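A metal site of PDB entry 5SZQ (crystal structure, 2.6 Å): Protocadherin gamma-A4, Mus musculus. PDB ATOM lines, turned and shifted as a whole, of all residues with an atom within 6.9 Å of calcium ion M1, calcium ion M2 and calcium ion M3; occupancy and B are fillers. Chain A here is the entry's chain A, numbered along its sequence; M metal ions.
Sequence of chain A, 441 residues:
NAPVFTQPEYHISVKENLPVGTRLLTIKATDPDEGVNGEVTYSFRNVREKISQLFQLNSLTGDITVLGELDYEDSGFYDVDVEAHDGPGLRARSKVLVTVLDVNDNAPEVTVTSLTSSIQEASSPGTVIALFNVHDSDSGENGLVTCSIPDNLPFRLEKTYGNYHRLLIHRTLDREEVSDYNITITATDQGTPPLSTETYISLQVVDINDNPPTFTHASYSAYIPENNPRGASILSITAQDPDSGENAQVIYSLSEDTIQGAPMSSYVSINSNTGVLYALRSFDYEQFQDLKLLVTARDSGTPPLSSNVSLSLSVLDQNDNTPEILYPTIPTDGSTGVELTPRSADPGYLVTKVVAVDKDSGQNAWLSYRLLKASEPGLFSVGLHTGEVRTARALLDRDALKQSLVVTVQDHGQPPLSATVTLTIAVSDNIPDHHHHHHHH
O of Glu 121 sits close to O of Leu 173, at 2.7 Å.
O of Asp 243 sits close to NH1 of Arg 175 (3.0 Å).
The side-chain amide oxygen (OD1) of Asn 211 lies close to the side-chain carboxylate (OD1) of Asp 210, 2.9 Å away.
OE2 of Glu 176 lies close to NH1 of Arg 175 (3.2 Å).
The backbone carbonyl oxygen (O) of Val 206 sits at hydrogen-bond distance from the backbone NH (N) of Glu 121 (3.4 Å).
OE1 of Glu 176 lies close to OD2 of Asp 174 (2.7 Å).
NH1 of Arg 175 sits close to OD1 of Asp 207, at 3.8 Å.
OD2 of Asp 207 is in hydrogen-bond range of N of Ser 244, at 3.2 Å.
Within 4 Å of calcium ion M1: Glu 121, Asp 174, Glu 176, Asp 210 and Asn 211.
Within 4 Å of calcium ion M2: Glu 121, Glu 176, Asp 207, Ile 208, Asp 210 and Asp 243.
Within 4 Å of calcium ion M3: Asn 209, Asn 211, Asp 241, Asp 243, Asn 247 and Asp 299.
Calcium ion M1 is bound by the side-chain carboxylate (OD2) of Asp 210 (2.5 Å), the side-chain carboxylate (OD2) of Asp 174 (2.5 Å) and the side-chain carboxylate (OE1) of Glu 121 (2.6 Å).
Slightly farther from calcium ion M1 lies OE1 of Glu 176 (3.1 Å).
Slightly farther from calcium ion M1 lies the side-chain carboxylate (OD1) of Asp 174 (3.1 Å).
OE2 of Glu 176 is bound to calcium ion M2.
Calcium ion M2 is bound by OD1 of Asp 207.
Calcium ion M2 is bound by O of Ile 208 (2.4 Å).
Calcium ion M2 is bound by OE2 of Glu 121, 2.6 Å away.
OD1 of Asp 243 is bound to calcium ion M2 (2.8 Å).
Slightly farther from calcium ion M2 lies the side-chain carboxylate (OD1) of Asp 210 (3.0 Å).
Slightly farther from calcium ion M2 lies the side-chain carboxylate (OE1) of Glu 176 (3.0 Å).
Calcium ion M3 is bound by the side-chain amide oxygen (OD1) of Asn 209 (2.4 Å), the backbone carbonyl oxygen (O) of Asn 211 (2.4 Å), the backbone carbonyl oxygen (O) of Asn 247 (2.4 Å), the side-chain carboxylate (OD2) of Asp 241 (2.5 Å), the side-chain carboxylate (OD2) of Asp 299 (2.6 Å) and the side-chain carboxylate (OD2) of Asp 243 (2.8 Å).
Slightly farther from calcium ion M3 lies OD1 of Asp 241 (2.9 Å).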
ATOM      1  N   GLU A 121      -6.328 -29.238  -8.330  1.00  0.00           N
ATOM      2  CA  GLU A 121      -6.328 -29.099  -9.786  1.00  0.00           C
ATOM      3  C   GLU A 121      -4.967 -29.466 -10.364  1.00  0.00           C
ATOM      4  O   GLU A 121      -4.843 -30.475 -11.069  1.00  0.00           O
ATOM      5  CB  GLU A 121      -6.718 -27.660 -10.159  1.00  0.00           C
ATOM      6  CG  GLU A 121      -6.950 -27.455 -11.650  1.00  0.00           C
ATOM      7  CD  GLU A 121      -7.383 -26.048 -12.000  1.00  0.00           C
ATOM      8  OE1 GLU A 121      -6.771 -25.447 -12.904  1.00  0.00           O
ATOM      9  OE2 GLU A 121      -8.339 -25.547 -11.363  1.00  0.00           O
ATOM     10  N   LEU A 173      -5.284 -33.820 -14.096  1.00  0.00           N
ATOM     11  CA  LEU A 173      -6.646 -33.353 -13.905  1.00  0.00           C
ATOM     12  C   LEU A 173      -6.681 -31.828 -13.920  1.00  0.00           C
ATOM     13  O   LEU A 173      -5.732 -31.166 -13.488  1.00  0.00           O
ATOM     14  CB  LEU A 173      -7.206 -33.894 -12.583  1.00  0.00           C
ATOM     15  CG  LEU A 173      -8.708 -33.811 -12.295  1.00  0.00           C
ATOM     16  CD1 LEU A 173      -9.055 -32.480 -11.669  1.00  0.00           C
ATOM     17  CD2 LEU A 173      -9.526 -34.063 -13.557  1.00  0.00           C
ATOM     18  N   ASP A 174      -7.785 -31.263 -14.432  1.00  0.00           N
ATOM     19  CA  ASP A 174      -7.967 -29.817 -14.521  1.00  0.00           C
ATOM     20  C   ASP A 174      -9.432 -29.489 -14.255  1.00  0.00           C
ATOM     21  O   ASP A 174     -10.312 -30.008 -14.946  1.00  0.00           O
ATOM     22  CB  ASP A 174      -7.537 -29.283 -15.898  1.00  0.00           C
ATOM     23  CG  ASP A 174      -7.703 -27.763 -16.019  1.00  0.00           C
ATOM     24  OD1 ASP A 174      -7.727 -27.251 -17.163  1.00  0.00           O
ATOM     25  OD2 ASP A 174      -7.803 -27.093 -14.970  1.00  0.00           O
ATOM     26  N   ARG A 175      -9.674 -28.625 -13.277  1.00  0.00           N
ATOM     27  CA  ARG A 175     -11.043 -28.365 -12.815  1.00  0.00           C
ATOM     28  C   ARG A 175     -11.893 -27.697 -13.890  1.00  0.00           C
ATOM     29  O   ARG A 175     -13.118 -27.863 -13.896  1.00  0.00           O
ATOM     30  CB  ARG A 175     -10.992 -27.505 -11.551  1.00  0.00           C
ATOM     31  CG  ARG A 175     -12.331 -27.143 -10.980  1.00  0.00           C
ATOM     32  CD  ARG A 175     -12.641 -25.692 -11.274  1.00  0.00           C
ATOM     33  NE  ARG A 175     -14.062 -25.464 -11.506  1.00  0.00           N
ATOM     34  CZ  ARG A 175     -14.574 -24.323 -11.962  1.00  0.00           C
ATOM     35  NH1 ARG A 175     -13.768 -23.307 -12.234  1.00  0.00           N
ATOM     36  NH2 ARG A 175     -15.878 -24.204 -12.158  1.00  0.00           N
ATOM     37  N   GLU A 176     -11.276 -26.956 -14.814  1.00  0.00           N
ATOM     38  CA  GLU A 176     -12.026 -26.187 -15.800  1.00  0.00           C
ATOM     39  C   GLU A 176     -12.721 -27.054 -16.853  1.00  0.00           C
ATOM     40  O   GLU A 176     -13.427 -26.504 -17.696  1.00  0.00           O
ATOM     41  CB  GLU A 176     -11.114 -25.165 -16.492  1.00  0.00           C
ATOM     42  CG  GLU A 176     -10.870 -23.900 -15.685  1.00  0.00           C
ATOM     43  CD  GLU A 176     -10.242 -24.176 -14.332  1.00  0.00           C
ATOM     44  OE1 GLU A 176      -9.238 -24.911 -14.284  1.00  0.00           O
ATOM     45  OE2 GLU A 176     -10.774 -23.674 -13.320  1.00  0.00           O
ATOM     46  N   GLU A 177     -12.529 -28.378 -16.831  1.00  0.00           N
ATOM     47  CA  GLU A 177     -13.214 -29.256 -17.770  1.00  0.00           C
ATOM     48  C   GLU A 177     -14.547 -29.744 -17.202  1.00  0.00           C
ATOM     49  O   GLU A 177     -15.608 -29.556 -17.823  1.00  0.00           O
ATOM     50  CB  GLU A 177     -12.328 -30.444 -18.150  1.00  0.00           C
ATOM     51  CG  GLU A 177     -11.379 -30.191 -19.316  1.00  0.00           C
ATOM     52  CD  GLU A 177     -10.291 -29.195 -18.967  1.00  0.00           C
ATOM     53  OE1 GLU A 177      -9.810 -28.493 -19.884  1.00  0.00           O
ATOM     54  OE2 GLU A 177      -9.922 -29.107 -17.776  1.00  0.00           O
ATOM     55  N   VAL A 206     -10.836 -29.665  -6.434  1.00  0.00           N
ATOM     56  CA  VAL A 206     -10.291 -28.414  -5.903  1.00  0.00           C
ATOM     57  C   VAL A 206      -9.936 -27.496  -7.064  1.00  0.00           C
ATOM     58  O   VAL A 206      -9.481 -27.947  -8.129  1.00  0.00           O
ATOM     59  CB  VAL A 206      -9.069 -28.707  -5.009  1.00  0.00           C
ATOM     60  CG1 VAL A 206      -8.527 -27.431  -4.402  1.00  0.00           C
ATOM     61  CG2 VAL A 206      -9.444 -29.710  -3.928  1.00  0.00           C
ATOM     62  N   ASP A 207     -10.164 -26.191  -6.872  1.00  0.00           N
ATOM     63  CA  ASP A 207     -10.036 -25.184  -7.916  1.00  0.00           C
ATOM     64  C   ASP A 207      -8.893 -24.232  -7.561  1.00  0.00           C
ATOM     65  O   ASP A 207      -8.998 -23.471  -6.593  1.00  0.00           O
ATOM     66  CB  ASP A 207     -11.347 -24.424  -8.086  1.00  0.00           C
ATOM     67  CG  ASP A 207     -11.228 -23.231  -9.004  1.00  0.00           C
ATOM     68  OD1 ASP A 207     -10.619 -23.377 -10.085  1.00  0.00           O
ATOM     69  OD2 ASP A 207     -11.737 -22.147  -8.665  1.00  0.00           O
ATOM     70  N   ILE A 208      -7.802 -24.285  -8.344  1.00  0.00           N
ATOM     71  CA  ILE A 208      -6.688 -23.348  -8.202  1.00  0.00           C
ATOM     72  C   ILE A 208      -6.976 -22.116  -9.053  1.00  0.00           C
ATOM     73  O   ILE A 208      -7.630 -22.187 -10.096  1.00  0.00           O
ATOM     74  CB  ILE A 208      -5.342 -23.999  -8.611  1.00  0.00           C
ATOM     75  CG1 ILE A 208      -5.054 -25.223  -7.748  1.00  0.00           C
ATOM     76  CG2 ILE A 208      -4.184 -23.005  -8.491  1.00  0.00           C
ATOM     77  CD1 ILE A 208      -3.653 -25.765  -7.944  1.00  0.00           C
ATOM     78  N   ASN A 209      -6.486 -20.961  -8.585  1.00  0.00           N
ATOM     79  CA  ASN A 209      -6.592 -19.715  -9.331  1.00  0.00           C
ATOM     80  C   ASN A 209      -5.439 -19.632 -10.327  1.00  0.00           C
ATOM     81  O   ASN A 209      -4.447 -18.921 -10.137  1.00  0.00           O
ATOM     82  CB  ASN A 209      -6.580 -18.526  -8.371  1.00  0.00           C
ATOM     83  CG  ASN A 209      -6.887 -17.212  -9.055  1.00  0.00           C
ATOM     84  OD1 ASN A 209      -7.578 -17.185 -10.073  1.00  0.00           O
ATOM     85  ND2 ASN A 209      -6.369 -16.121  -8.498  1.00  0.00           N
ATOM     86  N   ASP A 210      -5.578 -20.374 -11.425  1.00  0.00           N
ATOM     87  CA  ASP A 210      -4.546 -20.439 -12.456  1.00  0.00           C
ATOM     88  C   ASP A 210      -4.965 -19.785 -13.765  1.00  0.00           C
ATOM     89  O   ASP A 210      -4.143 -19.704 -14.682  1.00  0.00           O
ATOM     90  CB  ASP A 210      -4.135 -21.900 -12.704  1.00  0.00           C
ATOM     91  CG  ASP A 210      -5.272 -22.749 -13.233  1.00  0.00           C
ATOM     92  OD1 ASP A 210      -6.446 -22.368 -13.042  1.00  0.00           O
ATOM     93  OD2 ASP A 210      -4.991 -23.812 -13.830  1.00  0.00           O
ATOM     94  N   ASN A 211      -6.217 -19.326 -13.885  1.00  0.00           N
ATOM     95  CA  ASN A 211      -6.686 -18.604 -15.049  1.00  0.00           C
ATOM     96  C   ASN A 211      -6.987 -17.150 -14.695  1.00  0.00           C
ATOM     97  O   ASN A 211      -7.571 -16.885 -13.632  1.00  0.00           O
ATOM     98  CB  ASN A 211      -7.937 -19.244 -15.644  1.00  0.00           C
ATOM     99  CG  ASN A 211      -7.702 -20.658 -16.144  1.00  0.00           C
ATOM    100  OD1 ASN A 211      -6.774 -21.334 -15.703  1.00  0.00           O
ATOM    101  ND2 ASN A 211      -8.552 -21.113 -17.053  1.00  0.00           N
ATOM    102  N   PRO A 212      -6.599 -16.191 -15.525  1.00  0.00           N
ATOM    103  CA  PRO A 212      -6.956 -14.798 -15.271  1.00  0.00           C
ATOM    104  C   PRO A 212      -8.287 -14.452 -15.916  1.00  0.00           C
ATOM    105  O   PRO A 212      -8.800 -15.218 -16.743  1.00  0.00           O
ATOM    106  CB  PRO A 212      -5.805 -14.022 -15.932  1.00  0.00           C
ATOM    107  CG  PRO A 212      -5.413 -14.899 -17.077  1.00  0.00           C
ATOM    108  CD  PRO A 212      -5.621 -16.320 -16.621  1.00  0.00           C
ATOM    109  N   PRO A 213      -8.885 -13.321 -15.542  1.00  0.00           N
ATOM    110  CA  PRO A 213     -10.085 -12.847 -16.259  1.00  0.00           C
ATOM    111  C   PRO A 213      -9.725 -12.310 -17.633  1.00  0.00           C
ATOM    112  O   PRO A 213      -8.770 -11.538 -17.780  1.00  0.00           O
ATOM    113  CB  PRO A 213     -10.645 -11.752 -15.339  1.00  0.00           C
ATOM    114  CG  PRO A 213      -9.480 -11.319 -14.511  1.00  0.00           C
ATOM    115  CD  PRO A 213      -8.619 -12.530 -14.324  1.00  0.00           C
ATOM    116  N   ASP A 241     -13.858 -15.042 -16.166  1.00  0.00           N
ATOM    117  CA  ASP A 241     -12.832 -15.870 -15.569  1.00  0.00           C
ATOM    118  C   ASP A 241     -13.309 -17.314 -15.499  1.00  0.00           C
ATOM    119  O   ASP A 241     -14.311 -17.599 -14.819  1.00  0.00           O
ATOM    120  CB  ASP A 241     -12.467 -15.368 -14.168  1.00  0.00           C
ATOM    121  CG  ASP A 241     -11.260 -16.093 -13.588  1.00  0.00           C
ATOM    122  OD1 ASP A 241     -10.266 -16.263 -14.334  1.00  0.00           O
ATOM    123  OD2 ASP A 241     -11.303 -16.506 -12.418  1.00  0.00           O
ATOM    124  N   PRO A 242     -12.643 -18.259 -16.176  1.00  0.00           N
ATOM    125  CA  PRO A 242     -13.142 -19.642 -16.218  1.00  0.00           C
ATOM    126  C   PRO A 242     -13.051 -20.381 -14.887  1.00  0.00           C
ATOM    127  O   PRO A 242     -13.398 -21.571 -14.841  1.00  0.00           O
ATOM    128  CB  PRO A 242     -12.243 -20.310 -17.274  1.00  0.00           C
ATOM    129  CG  PRO A 242     -11.625 -19.180 -18.049  1.00  0.00           C
ATOM    130  CD  PRO A 242     -11.489 -18.063 -17.068  1.00  0.00           C
ATOM    131  N   ASP A 243     -12.599 -19.738 -13.805  1.00  0.00           N
ATOM    132  CA  ASP A 243     -12.465 -20.418 -12.529  1.00  0.00           C
ATOM    133  C   ASP A 243     -13.793 -20.438 -11.778  1.00  0.00           C
ATOM    134  O   ASP A 243     -14.858 -20.524 -12.386  1.00  0.00           O
ATOM    135  CB  ASP A 243     -11.382 -19.766 -11.674  1.00  0.00           C
ATOM    136  CG  ASP A 243     -10.004 -19.849 -12.306  1.00  0.00           C
ATOM    137  OD1 ASP A 243      -9.788 -20.778 -13.124  1.00  0.00           O
ATOM    138  OD2 ASP A 243      -9.143 -19.008 -11.988  1.00  0.00           O
ATOM    139  N   SER A 244     -13.739 -20.365 -10.450  1.00  0.00           N
ATOM    140  CA  SER A 244     -14.947 -20.447  -9.642  1.00  0.00           C
ATOM    141  C   SER A 244     -14.683 -19.795  -8.287  1.00  0.00           C
ATOM    142  O   SER A 244     -13.536 -19.619  -7.873  1.00  0.00           O
ATOM    143  CB  SER A 244     -15.407 -21.897  -9.469  1.00  0.00           C
ATOM    144  OG  SER A 244     -16.664 -21.976  -8.828  1.00  0.00           O
ATOM    145  N   GLU A 246     -14.186 -17.362  -5.170  1.00  0.00           N
ATOM    146  CA  GLU A 246     -13.462 -16.109  -5.027  1.00  0.00           C
ATOM    147  C   GLU A 246     -12.485 -15.899  -6.167  1.00  0.00           C
ATOM    148  O   GLU A 246     -12.334 -14.784  -6.680  1.00  0.00           O
ATOM    149  CB  GLU A 246     -12.735 -16.070  -3.676  1.00  0.00           C
ATOM    150  CG  GLU A 246     -13.318 -15.091  -2.658  1.00  0.00           C
ATOM    151  CD  GLU A 246     -12.414 -14.917  -1.461  1.00  0.00           C
ATOM    152  OE1 GLU A 246     -11.268 -15.412  -1.496  1.00  0.00           O
ATOM    153  OE2 GLU A 246     -12.843 -14.295  -0.462  1.00  0.00           O
ATOM    154  N   ASN A 247     -11.823 -16.968  -6.609  1.00  0.00           N
ATOM    155  CA  ASN A 247     -10.829 -16.906  -7.683  1.00  0.00           C
ATOM    156  C   ASN A 247     -11.410 -16.509  -9.031  1.00  0.00           C
ATOM    157  O   ASN A 247     -10.652 -16.410  -9.997  1.00  0.00           O
ATOM    158  CB  ASN A 247     -10.119 -18.253  -7.795  1.00  0.00           C
ATOM    159  CG  ASN A 247      -9.428 -18.660  -6.515  1.00  0.00           C
ATOM    160  OD1 ASN A 247      -8.873 -17.824  -5.800  1.00  0.00           O
ATOM    161  ND2 ASN A 247      -9.438 -19.957  -6.214  1.00  0.00           N
ATOM    162  N   ALA A 248     -12.720 -16.281  -9.127  1.00  0.00           N
ATOM    163  CA  ALA A 248     -13.352 -15.972 -10.409  1.00  0.00           C
ATOM    164  C   ALA A 248     -14.162 -14.691 -10.425  1.00  0.00           C
ATOM    165  O   ALA A 248     -14.655 -14.309 -11.493  1.00  0.00           O
ATOM    166  CB  ALA A 248     -14.265 -17.117 -10.858  1.00  0.00           C
ATOM    167  N   GLN A 249     -14.329 -14.015  -9.293  1.00  0.00           N
ATOM    168  CA  GLN A 249     -14.953 -12.702  -9.290  1.00  0.00           C
ATOM    169  C   GLN A 249     -14.131 -11.726 -10.115  1.00  0.00           C
ATOM    170  O   GLN A 249     -12.916 -11.867 -10.242  1.00  0.00           O
ATOM    171  CB  GLN A 249     -15.095 -12.179  -7.855  1.00  0.00           C
ATOM    172  CG  GLN A 249     -15.924 -13.078  -6.945  1.00  0.00           C
ATOM    173  CD  GLN A 249     -16.010 -12.524  -5.533  1.00  0.00           C
ATOM    174  OE1 GLN A 249     -15.494 -11.446  -5.243  1.00  0.00           O
ATOM    175  NE2 GLN A 249     -16.677 -13.257  -4.652  1.00  0.00           N
ATOM    176  N   ARG A 298      -9.321  -7.619 -12.114  1.00  0.00           N
ATOM    177  CA  ARG A 298      -8.673  -8.578 -11.229  1.00  0.00           C
ATOM    178  C   ARG A 298      -9.713  -9.516 -10.615  1.00  0.00           C
ATOM    179  O   ARG A 298     -10.918  -9.368 -10.835  1.00  0.00           O
ATOM    180  CB  ARG A 298      -7.883  -7.849 -10.129  1.00  0.00           C
ATOM    181  CG  ARG A 298      -8.753  -7.089  -9.132  1.00  0.00           C
ATOM    182  CD  ARG A 298      -7.919  -6.549  -7.975  1.00  0.00           C
ATOM    183  NE  ARG A 298      -8.733  -5.788  -7.032  1.00  0.00           N
ATOM    184  CZ  ARG A 298      -9.373  -6.318  -5.996  1.00  0.00           C
ATOM    185  NH1 ARG A 298     -10.099  -5.550  -5.188  1.00  0.00           N
ATOM    186  NH2 ARG A 298      -9.293  -7.621  -5.756  1.00  0.00           N
ATOM    187  N   ASP A 299      -9.233 -10.498  -9.848  1.00  0.00           N
ATOM    188  CA  ASP A 299     -10.090 -11.406  -9.104  1.00  0.00           C
ATOM    189  C   ASP A 299      -9.808 -11.282  -7.613  1.00  0.00           C
ATOM    190  O   ASP A 299      -8.793 -10.721  -7.189  1.00  0.00           O
ATOM    191  CB  ASP A 299      -9.920 -12.865  -9.565  1.00  0.00           C
ATOM    192  CG  ASP A 299      -8.499 -13.392  -9.396  1.00  0.00           C
ATOM    193  OD1 ASP A 299      -7.630 -12.675  -8.878  1.00  0.00           O
ATOM    194  OD2 ASP A 299      -8.257 -14.555  -9.795  1.00  0.00           O
ATOM    195  N   SER A 300     -10.739 -11.802  -6.816  1.00  0.00           N
ATOM    196  CA  SER A 300     -10.597 -11.780  -5.361  1.00  0.00           C
ATOM    197  C   SER A 300      -9.668 -12.910  -4.929  1.00  0.00           C
ATOM    198  O   SER A 300      -9.037 -13.584  -5.740  1.00  0.00           O
ATOM    199  CB  SER A 300     -11.974 -11.859  -4.704  1.00  0.00           C
ATOM    200  OG  SER A 300     -12.814 -10.802  -5.138  1.00  0.00           O
ATOM    201  N   LEU A 305      -5.274 -11.904  -9.525  1.00  0.00           N
ATOM    202  CA  LEU A 305      -4.820 -12.150 -10.884  1.00  0.00           C
ATOM    203  C   LEU A 305      -5.665 -11.305 -11.827  1.00  0.00           C
ATOM    204  O   LEU A 305      -6.896 -11.426 -11.837  1.00  0.00           O
ATOM    205  CB  LEU A 305      -4.945 -13.634 -11.244  1.00  0.00           C
ATOM    206  CG  LEU A 305      -4.487 -14.108 -12.628  1.00  0.00           C
ATOM    207  CD1 LEU A 305      -3.116 -13.559 -12.985  1.00  0.00           C
ATOM    208  CD2 LEU A 305      -4.484 -15.634 -12.711  1.00  0.00           C
HETATM  209 CA    CA M   1      -6.399 -25.025 -15.443  1.00  0.00          CA
HETATM  210 CA    CA M   2      -9.087 -23.130 -11.824  1.00  0.00          CA
HETATM  211 CA    CA M   3      -8.938 -16.212 -11.734  1.00  0.00          CA
